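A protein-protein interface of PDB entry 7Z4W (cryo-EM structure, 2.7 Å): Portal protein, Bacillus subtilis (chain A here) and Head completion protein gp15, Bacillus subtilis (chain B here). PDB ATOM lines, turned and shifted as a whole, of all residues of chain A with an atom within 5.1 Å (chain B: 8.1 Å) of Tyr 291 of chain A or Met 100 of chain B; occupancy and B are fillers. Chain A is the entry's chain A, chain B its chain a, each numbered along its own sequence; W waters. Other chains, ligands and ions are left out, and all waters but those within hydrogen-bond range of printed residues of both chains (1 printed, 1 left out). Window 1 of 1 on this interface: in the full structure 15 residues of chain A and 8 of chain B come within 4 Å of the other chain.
Water W1 lies within hydrogen-bond range of the backbone carbonyl oxygen of Lys 310 of chain A (3.0 Å) and the backbone NH of Ala 101 of chain B (3.3 Å).
Of the printed residues of chain B, Leu 288 of chain A touches Met 100 (3.9 Å).
Of the printed residues of chain B, Asp 292 of chain A touches Pro 96 and Arg 98.
Printed residues of chain A within 4 Å of Lys 99 of chain B: Tyr 291 (3.5 Å) and Gly 293 (3.5 Å).
Printed residues of chain A within 4 Å of Ala 101 of chain B: Lys 310 (3.99 Å).
The nearest residue of chain B that does not touch Tyr 291 of chain A is Asn 95 of chain B (5.7 Å).
OD1 of Asn 290 of chain A lies within hydrogen-bond range of ND2 of Asn 95 of chain B, at 3.3 Å.
The backbone carbonyl oxygen of Asn 290 of chain A lies within hydrogen-bond range of the guanidinium group of Arg 98 of chain B, at 3.0 Å.
N of Asp 292 of chain A sits at hydrogen-bond distance from O of Arg 98 of chain B (3.4 Å).
The backbone NH (N) of Gly 293 of chain A lies within hydrogen-bond range of the backbone carbonyl oxygen (O) of Arg 98 of chain B (3.1 Å).
OE1 of Glu 294 of chain A lies within hydrogen-bond range of N of Met 100 of chain B (3.2 Å).
O of Ser 312 of chain A sits at hydrogen-bond distance from NH2 of Arg 98 of chain B (3.3 Å).
Of the 14 printed residues of chain A, 12 touch a printed residue of chain B.
Printed residues of chain A that touch a printed residue of chain B: Leu 288, Asn 290, Tyr 291, Asp 292, Gly 293, Glu 294, Phe 299, Ile 309, Lys 310, Val 311, Ser 312 and Gly 315.
Hydrophobic or aromatic side chains of chain B that line the printed part of chain A: Met 100.
Among the printed residues, no Asp or Glu carboxylate lies within 4 Å of a Lys or Arg side-chain nitrogen of the other chain.
The backbone NH of Ser 312 of chain A sits at hydrogen-bond distance from the side-chain hydroxyl of Tyr 291 of chain A.
The guanidinium group of Arg 98 of chain B is in salt-bridge range of the side-chain carboxylate of Glu 35 of chain B (3.3 Å).
The backbone NH of Lys 99 of chain B lies within hydrogen-bond range of the backbone carbonyl oxygen of Cys 36 of chain B (2.9 Å).
CD2 of Leu 288 of chain A touches CE of Met 100 of chain B, 3.9 Å away.
Tyr 291 of chain A touches Arg 98 of chain B.
Lys 99 of chain B touches Tyr 291 of chain A.
Pro 96 of chain B touches Asp 292 of chain A (O to CB, 3.8 Å).
Lys 99 of chain B touches Gly 293 of chain A.
Phe 299 of chain A touches Met 100 of chain B.
Ile 309 of chain A touches Met 100 of chain B.
Arg 102 of chain B touches Lys 310 of chain A (O to NZ, 3.5 Å).
Val 311 of chain A touches Met 100 of chain B.
Arg 98 of chain B touches Gly 315 of chain A.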
ATOM      1  N   LEU A 288      10.861 -21.520  12.951  1.00  0.00           N
ATOM      2  CA  LEU A 288       9.543 -22.135  13.059  1.00  0.00           C
ATOM      3  C   LEU A 288       8.495 -21.071  13.368  1.00  0.00           C
ATOM      4  O   LEU A 288       8.689 -20.250  14.268  1.00  0.00           O
ATOM      5  CB  LEU A 288       9.535 -23.209  14.149  1.00  0.00           C
ATOM      6  CG  LEU A 288      10.202 -24.547  13.828  1.00  0.00           C
ATOM      7  CD1 LEU A 288      10.125 -25.484  15.018  1.00  0.00           C
ATOM      8  CD2 LEU A 288       9.574 -25.185  12.605  1.00  0.00           C
ATOM      9  N   LYS A 289       7.381 -21.097  12.635  1.00  0.00           N
ATOM     10  CA  LYS A 289       6.307 -20.121  12.772  1.00  0.00           C
ATOM     11  C   LYS A 289       5.051 -20.812  13.281  1.00  0.00           C
ATOM     12  O   LYS A 289       4.537 -21.724  12.622  1.00  0.00           O
ATOM     13  CB  LYS A 289       6.025 -19.428  11.439  1.00  0.00           C
ATOM     14  CG  LYS A 289       7.014 -18.342  11.090  1.00  0.00           C
ATOM     15  CD  LYS A 289       7.148 -18.169   9.583  1.00  0.00           C
ATOM     16  CE  LYS A 289       7.955 -19.293   8.951  1.00  0.00           C
ATOM     17  NZ  LYS A 289       9.204 -19.572   9.704  1.00  0.00           N
ATOM     18  N   ASN A 290       4.580 -20.370  14.457  1.00  0.00           N
ATOM     19  CA  ASN A 290       3.341 -20.819  15.118  1.00  0.00           C
ATOM     20  C   ASN A 290       3.392 -22.295  15.517  1.00  0.00           C
ATOM     21  O   ASN A 290       2.419 -23.030  15.357  1.00  0.00           O
ATOM     22  CB  ASN A 290       2.094 -20.528  14.271  1.00  0.00           C
ATOM     23  CG  ASN A 290       1.863 -19.052  14.060  1.00  0.00           C
ATOM     24  OD1 ASN A 290       1.816 -18.283  15.009  1.00  0.00           O
ATOM     25  ND2 ASN A 290       1.718 -18.651  12.813  1.00  0.00           N
ATOM     26  N   TYR A 291       4.542 -22.736  16.053  1.00  0.00           N
ATOM     27  CA  TYR A 291       4.671 -24.050  16.698  1.00  0.00           C
ATOM     28  C   TYR A 291       5.440 -23.841  18.002  1.00  0.00           C
ATOM     29  O   TYR A 291       6.650 -24.037  18.067  1.00  0.00           O
ATOM     30  CB  TYR A 291       5.379 -25.062  15.795  1.00  0.00           C
ATOM     31  CG  TYR A 291       4.563 -25.531  14.620  1.00  0.00           C
ATOM     32  CD1 TYR A 291       3.488 -26.392  14.798  1.00  0.00           C
ATOM     33  CD2 TYR A 291       4.862 -25.105  13.332  1.00  0.00           C
ATOM     34  CE1 TYR A 291       2.737 -26.818  13.729  1.00  0.00           C
ATOM     35  CE2 TYR A 291       4.117 -25.526  12.257  1.00  0.00           C
ATOM     36  CZ  TYR A 291       3.055 -26.381  12.461  1.00  0.00           C
ATOM     37  OH  TYR A 291       2.310 -26.802  11.391  1.00  0.00           O
ATOM     38  N   ASP A 292       4.727 -23.491  19.065  1.00  0.00           N
ATOM     39  CA  ASP A 292       5.381 -23.132  20.316  1.00  0.00           C
ATOM     40  C   ASP A 292       5.584 -24.312  21.257  1.00  0.00           C
ATOM     41  O   ASP A 292       6.346 -24.185  22.218  1.00  0.00           O
ATOM     42  CB  ASP A 292       4.590 -22.040  21.037  1.00  0.00           C
ATOM     43  CG  ASP A 292       4.939 -20.649  20.554  1.00  0.00           C
ATOM     44  OD1 ASP A 292       5.858 -20.505  19.723  1.00  0.00           O
ATOM     45  OD2 ASP A 292       4.289 -19.689  21.007  1.00  0.00           O
ATOM     46  N   GLY A 293       4.936 -25.443  21.011  1.00  0.00           N
ATOM     47  CA  GLY A 293       5.143 -26.626  21.815  1.00  0.00           C
ATOM     48  C   GLY A 293       6.181 -27.601  21.309  1.00  0.00           C
ATOM     49  O   GLY A 293       6.375 -28.649  21.929  1.00  0.00           O
ATOM     50  N   GLU A 294       6.864 -27.289  20.213  1.00  0.00           N
ATOM     51  CA  GLU A 294       7.756 -28.237  19.555  1.00  0.00           C
ATOM     52  C   GLU A 294       9.114 -28.313  20.252  1.00  0.00           C
ATOM     53  O   GLU A 294       9.712 -27.287  20.583  1.00  0.00           O
ATOM     54  CB  GLU A 294       7.928 -27.843  18.086  1.00  0.00           C
ATOM     55  CG  GLU A 294       8.815 -28.755  17.248  1.00  0.00           C
ATOM     56  CD  GLU A 294       8.218 -30.131  17.011  1.00  0.00           C
ATOM     57  OE1 GLU A 294       6.979 -30.270  17.046  1.00  0.00           O
ATOM     58  OE2 GLU A 294       8.995 -31.081  16.789  1.00  0.00           O
ATOM     59  N   PHE A 299      12.941 -32.194  16.670  1.00  0.00           N
ATOM     60  CA  PHE A 299      12.621 -31.610  15.369  1.00  0.00           C
ATOM     61  C   PHE A 299      13.778 -31.761  14.382  1.00  0.00           C
ATOM     62  O   PHE A 299      13.582 -32.224  13.252  1.00  0.00           O
ATOM     63  CB  PHE A 299      12.229 -30.138  15.546  1.00  0.00           C
ATOM     64  CG  PHE A 299      12.234 -29.339  14.273  1.00  0.00           C
ATOM     65  CD1 PHE A 299      11.210 -29.480  13.350  1.00  0.00           C
ATOM     66  CD2 PHE A 299      13.245 -28.424  14.011  1.00  0.00           C
ATOM     67  CE1 PHE A 299      11.207 -28.748  12.179  1.00  0.00           C
ATOM     68  CE2 PHE A 299      13.248 -27.690  12.842  1.00  0.00           C
ATOM     69  CZ  PHE A 299      12.225 -27.850  11.927  1.00  0.00           C
ATOM     70  N   ILE A 309       9.151 -32.339   6.108  1.00  0.00           N
ATOM     71  CA  ILE A 309       8.555 -31.501   7.144  1.00  0.00           C
ATOM     72  C   ILE A 309       7.074 -31.327   6.821  1.00  0.00           C
ATOM     73  O   ILE A 309       6.717 -31.049   5.673  1.00  0.00           O
ATOM     74  CB  ILE A 309       9.271 -30.133   7.232  1.00  0.00           C
ATOM     75  CG1 ILE A 309      10.690 -30.293   7.765  1.00  0.00           C
ATOM     76  CG2 ILE A 309       8.528 -29.152   8.129  1.00  0.00           C
ATOM     77  CD1 ILE A 309      11.570 -29.122   7.427  1.00  0.00           C
ATOM     78  N   LYS A 310       6.215 -31.499   7.828  1.00  0.00           N
ATOM     79  CA  LYS A 310       4.772 -31.326   7.687  1.00  0.00           C
ATOM     80  C   LYS A 310       4.310 -30.073   8.421  1.00  0.00           C
ATOM     81  O   LYS A 310       4.526 -29.946   9.629  1.00  0.00           O
ATOM     82  CB  LYS A 310       4.020 -32.540   8.227  1.00  0.00           C
ATOM     83  CG  LYS A 310       4.412 -33.856   7.605  1.00  0.00           C
ATOM     84  CD  LYS A 310       3.293 -34.866   7.742  1.00  0.00           C
ATOM     85  CE  LYS A 310       3.693 -36.022   8.628  1.00  0.00           C
ATOM     86  NZ  LYS A 310       2.521 -36.820   9.065  1.00  0.00           N
ATOM     87  N   VAL A 311       3.664 -29.161   7.696  1.00  0.00           N
ATOM     88  CA  VAL A 311       3.064 -27.954   8.261  1.00  0.00           C
ATOM     89  C   VAL A 311       1.613 -27.868   7.802  1.00  0.00           C
ATOM     90  O   VAL A 311       1.245 -28.443   6.774  1.00  0.00           O
ATOM     91  CB  VAL A 311       3.835 -26.671   7.869  1.00  0.00           C
ATOM     92  CG1 VAL A 311       5.228 -26.661   8.478  1.00  0.00           C
ATOM     93  CG2 VAL A 311       3.891 -26.498   6.359  1.00  0.00           C
ATOM     94  N   SER A 312       0.782 -27.177   8.582  1.00  0.00           N
ATOM     95  CA  SER A 312      -0.610 -26.943   8.219  1.00  0.00           C
ATOM     96  C   SER A 312      -1.109 -25.650   8.850  1.00  0.00           C
ATOM     97  O   SER A 312      -0.606 -25.214   9.887  1.00  0.00           O
ATOM     98  CB  SER A 312      -1.517 -28.109   8.643  1.00  0.00           C
ATOM     99  OG  SER A 312      -1.309 -28.449   9.997  1.00  0.00           O
ATOM    100  N   GLY A 315       0.885 -22.394  10.373  1.00  0.00           N
ATOM    101  CA  GLY A 315       2.239 -22.772  10.709  1.00  0.00           C
ATOM    102  C   GLY A 315       3.156 -22.755   9.502  1.00  0.00           C
ATOM    103  O   GLY A 315       2.741 -22.976   8.369  1.00  0.00           O
ATOM    104  N   GLY A 316       4.432 -22.479   9.757  1.00  0.00           N
ATOM    105  CA  GLY A 316       5.385 -22.423   8.664  1.00  0.00           C
ATOM    106  C   GLY A 316       6.797 -22.698   9.126  1.00  0.00           C
ATOM    107  O   GLY A 316       7.081 -22.797  10.320  1.00  0.00           O
ATOM    108  N   GLU B  35      -5.976 -31.411  16.843  1.00  0.00           N
ATOM    109  CA  GLU B  35      -5.600 -30.234  16.074  1.00  0.00           C
ATOM    110  C   GLU B  35      -4.279 -29.646  16.554  1.00  0.00           C
ATOM    111  O   GLU B  35      -3.534 -29.083  15.748  1.00  0.00           O
ATOM    112  CB  GLU B  35      -6.727 -29.199  16.150  1.00  0.00           C
ATOM    113  CG  GLU B  35      -6.701 -28.118  15.082  1.00  0.00           C
ATOM    114  CD  GLU B  35      -5.885 -26.908  15.471  1.00  0.00           C
ATOM    115  OE1 GLU B  35      -5.763 -26.637  16.684  1.00  0.00           O
ATOM    116  OE2 GLU B  35      -5.372 -26.221  14.564  1.00  0.00           O
ATOM    117  N   CYS B  36      -3.964 -29.765  17.846  1.00  0.00           N
ATOM    118  CA  CYS B  36      -2.662 -29.314  18.321  1.00  0.00           C
ATOM    119  C   CYS B  36      -1.583 -30.390  18.260  1.00  0.00           C
ATOM    120  O   CYS B  36      -0.414 -30.062  18.488  1.00  0.00           O
ATOM    121  CB  CYS B  36      -2.767 -28.789  19.757  1.00  0.00           C
ATOM    122  SG  CYS B  36      -3.828 -27.351  19.961  1.00  0.00           S
ATOM    123  N   HIS B  37      -1.952 -31.641  17.945  1.00  0.00           N
ATOM    124  CA  HIS B  37      -1.075 -32.825  18.003  1.00  0.00           C
ATOM    125  C   HIS B  37      -0.426 -32.976  19.378  1.00  0.00           C
ATOM    126  O   HIS B  37       0.764 -33.261  19.502  1.00  0.00           O
ATOM    127  CB  HIS B  37      -0.018 -32.807  16.889  1.00  0.00           C
ATOM    128  CG  HIS B  37      -0.595 -32.770  15.508  1.00  0.00           C
ATOM    129  ND1 HIS B  37      -1.273 -33.834  14.955  1.00  0.00           N
ATOM    130  CD2 HIS B  37      -0.603 -31.793  14.572  1.00  0.00           C
ATOM    131  CE1 HIS B  37      -1.675 -33.513  13.739  1.00  0.00           C
ATOM    132  NE2 HIS B  37      -1.279 -32.281  13.483  1.00  0.00           N
ATOM    133  N   ASN B  38      -1.229 -32.800  20.419  1.00  0.00           N
ATOM    134  CA  ASN B  38      -0.769 -32.702  21.796  1.00  0.00           C
ATOM    135  C   ASN B  38      -1.715 -33.470  22.712  1.00  0.00           C
ATOM    136  O   ASN B  38      -2.889 -33.109  22.828  1.00  0.00           O
ATOM    137  CB  ASN B  38      -0.682 -31.229  22.206  1.00  0.00           C
ATOM    138  CG  ASN B  38       0.213 -30.989  23.406  1.00  0.00           C
ATOM    139  OD1 ASN B  38       0.373 -31.845  24.267  1.00  0.00           O
ATOM    140  ND2 ASN B  38       0.773 -29.796  23.482  1.00  0.00           N
ATOM    141  N   ASN B  95      -3.165 -21.583  20.019  1.00  0.00           N
ATOM    142  CA  ASN B  95      -1.840 -21.316  19.455  1.00  0.00           C
ATOM    143  C   ASN B  95      -0.631 -21.604  20.358  1.00  0.00           C
ATOM    144  O   ASN B  95       0.373 -22.100  19.820  1.00  0.00           O
ATOM    145  CB  ASN B  95      -1.786 -19.867  18.948  1.00  0.00           C
ATOM    146  CG  ASN B  95      -0.962 -19.719  17.687  1.00  0.00           C
ATOM    147  OD1 ASN B  95      -1.160 -20.441  16.714  1.00  0.00           O
ATOM    148  ND2 ASN B  95      -0.014 -18.793  17.706  1.00  0.00           N
ATOM    149  N   PRO B  96      -0.615 -21.328  21.675  1.00  0.00           N
ATOM    150  CA  PRO B  96       0.609 -21.624  22.443  1.00  0.00           C
ATOM    151  C   PRO B  96       0.904 -23.102  22.690  1.00  0.00           C
ATOM    152  O   PRO B  96       1.915 -23.396  23.335  1.00  0.00           O
ATOM    153  CB  PRO B  96       0.368 -20.899  23.776  1.00  0.00           C
ATOM    154  CG  PRO B  96      -0.610 -19.872  23.472  1.00  0.00           C
ATOM    155  CD  PRO B  96      -1.520 -20.507  22.509  1.00  0.00           C
ATOM    156  N   TYR B  97       0.098 -24.049  22.202  1.00  0.00           N
ATOM    157  CA  TYR B  97       0.314 -25.465  22.480  1.00  0.00           C
ATOM    158  C   TYR B  97       0.475 -26.304  21.217  1.00  0.00           C
ATOM    159  O   TYR B  97       0.331 -27.526  21.276  1.00  0.00           O
ATOM    160  CB  TYR B  97      -0.835 -26.025  23.317  1.00  0.00           C
ATOM    161  CG  TYR B  97      -1.269 -25.122  24.434  1.00  0.00           C
ATOM    162  CD1 TYR B  97      -0.482 -24.953  25.566  1.00  0.00           C
ATOM    163  CD2 TYR B  97      -2.461 -24.423  24.349  1.00  0.00           C
ATOM    164  CE1 TYR B  97      -0.877 -24.120  26.588  1.00  0.00           C
ATOM    165  CE2 TYR B  97      -2.862 -23.592  25.358  1.00  0.00           C
ATOM    166  CZ  TYR B  97      -2.073 -23.446  26.477  1.00  0.00           C
ATOM    167  OH  TYR B  97      -2.503 -22.603  27.474  1.00  0.00           O
ATOM    168  N   ARG B  98       0.776 -25.690  20.081  1.00  0.00           N
ATOM    169  CA  ARG B  98       0.775 -26.400  18.810  1.00  0.00           C
ATOM    170  C   ARG B  98       2.094 -27.132  18.590  1.00  0.00           C
ATOM    171  O   ARG B  98       3.170 -26.542  18.708  1.00  0.00           O
ATOM    172  CB  ARG B  98       0.510 -25.430  17.661  1.00  0.00           C
ATOM    173  CG  ARG B  98      -0.928 -24.970  17.572  1.00  0.00           C
ATOM    174  CD  ARG B  98      -1.087 -23.812  16.608  1.00  0.00           C
ATOM    175  NE  ARG B  98      -0.414 -24.057  15.337  1.00  0.00           N
ATOM    176  CZ  ARG B  98      -0.962 -24.698  14.312  1.00  0.00           C
ATOM    177  NH1 ARG B  98      -2.198 -25.164  14.401  1.00  0.00           N
ATOM    178  NH2 ARG B  98      -0.274 -24.872  13.195  1.00  0.00           N
ATOM    179  N   LYS B  99       2.000 -28.418  18.268  1.00  0.00           N
ATOM    180  CA  LYS B  99       3.132 -29.240  17.869  1.00  0.00           C
ATOM    181  C   LYS B  99       2.949 -29.681  16.424  1.00  0.00           C
ATOM    182  O   LYS B  99       1.897 -29.474  15.814  1.00  0.00           O
ATOM    183  CB  LYS B  99       3.283 -30.470  18.773  1.00  0.00           C
ATOM    184  CG  LYS B  99       3.517 -30.155  20.227  1.00  0.00           C
ATOM    185  CD  LYS B  99       3.491 -31.409  21.065  1.00  0.00           C
ATOM    186  CE  LYS B  99       4.000 -31.128  22.451  1.00  0.00           C
ATOM    187  NZ  LYS B  99       3.773 -32.266  23.364  1.00  0.00           N
ATOM    188  N   MET B 100       3.986 -30.302  15.878  1.00  0.00           N
ATOM    189  CA  MET B 100       3.952 -30.815  14.520  1.00  0.00           C
ATOM    190  C   MET B 100       3.572 -32.290  14.514  1.00  0.00           C
ATOM    191  O   MET B 100       3.856 -33.027  15.461  1.00  0.00           O
ATOM    192  CB  MET B 100       5.300 -30.620  13.829  1.00  0.00           C
ATOM    193  CG  MET B 100       5.619 -29.173  13.527  1.00  0.00           C
ATOM    194  SD  MET B 100       7.340 -28.883  13.088  1.00  0.00           S
ATOM    195  CE  MET B 100       7.128 -27.993  11.557  1.00  0.00           C
ATOM    196  N   ALA B 101       2.918 -32.707  13.435  1.00  0.00           N
ATOM    197  CA  ALA B 101       2.511 -34.097  13.289  1.00  0.00           C
ATOM    198  C   ALA B 101       3.718 -34.981  12.998  1.00  0.00           C
ATOM    199  O   ALA B 101       4.614 -34.608  12.239  1.00  0.00           O
ATOM    200  CB  ALA B 101       1.480 -34.237  12.173  1.00  0.00           C
ATOM    201  N   ARG B 102       3.740 -36.156  13.615  1.00  0.00           N
ATOM    202  CA  ARG B 102       4.833 -37.094  13.410  1.00  0.00           C
ATOM    203  C   ARG B 102       4.363 -38.320  12.636  1.00  0.00           C
ATOM    204  O   ARG B 102       4.585 -38.420  11.430  1.00  0.00           O
ATOM    205  CB  ARG B 102       5.443 -37.513  14.747  1.00  0.00           C
ATOM    206  CG  ARG B 102       6.308 -36.445  15.354  1.00  0.00           C
ATOM    207  CD  ARG B 102       6.967 -36.894  16.627  1.00  0.00           C
ATOM    208  NE  ARG B 102       7.673 -35.784  17.247  1.00  0.00           N
ATOM    209  CZ  ARG B 102       8.374 -35.872  18.366  1.00  0.00           C
ATOM    210  NH1 ARG B 102       8.475 -37.023  19.005  1.00  0.00           N
ATOM    211  NH2 ARG B 102       8.976 -34.798  18.847  1.00  0.00           N
HETATM  212  O   HOH W   1       2.098 -30.337  11.360  1.00  0.00           O
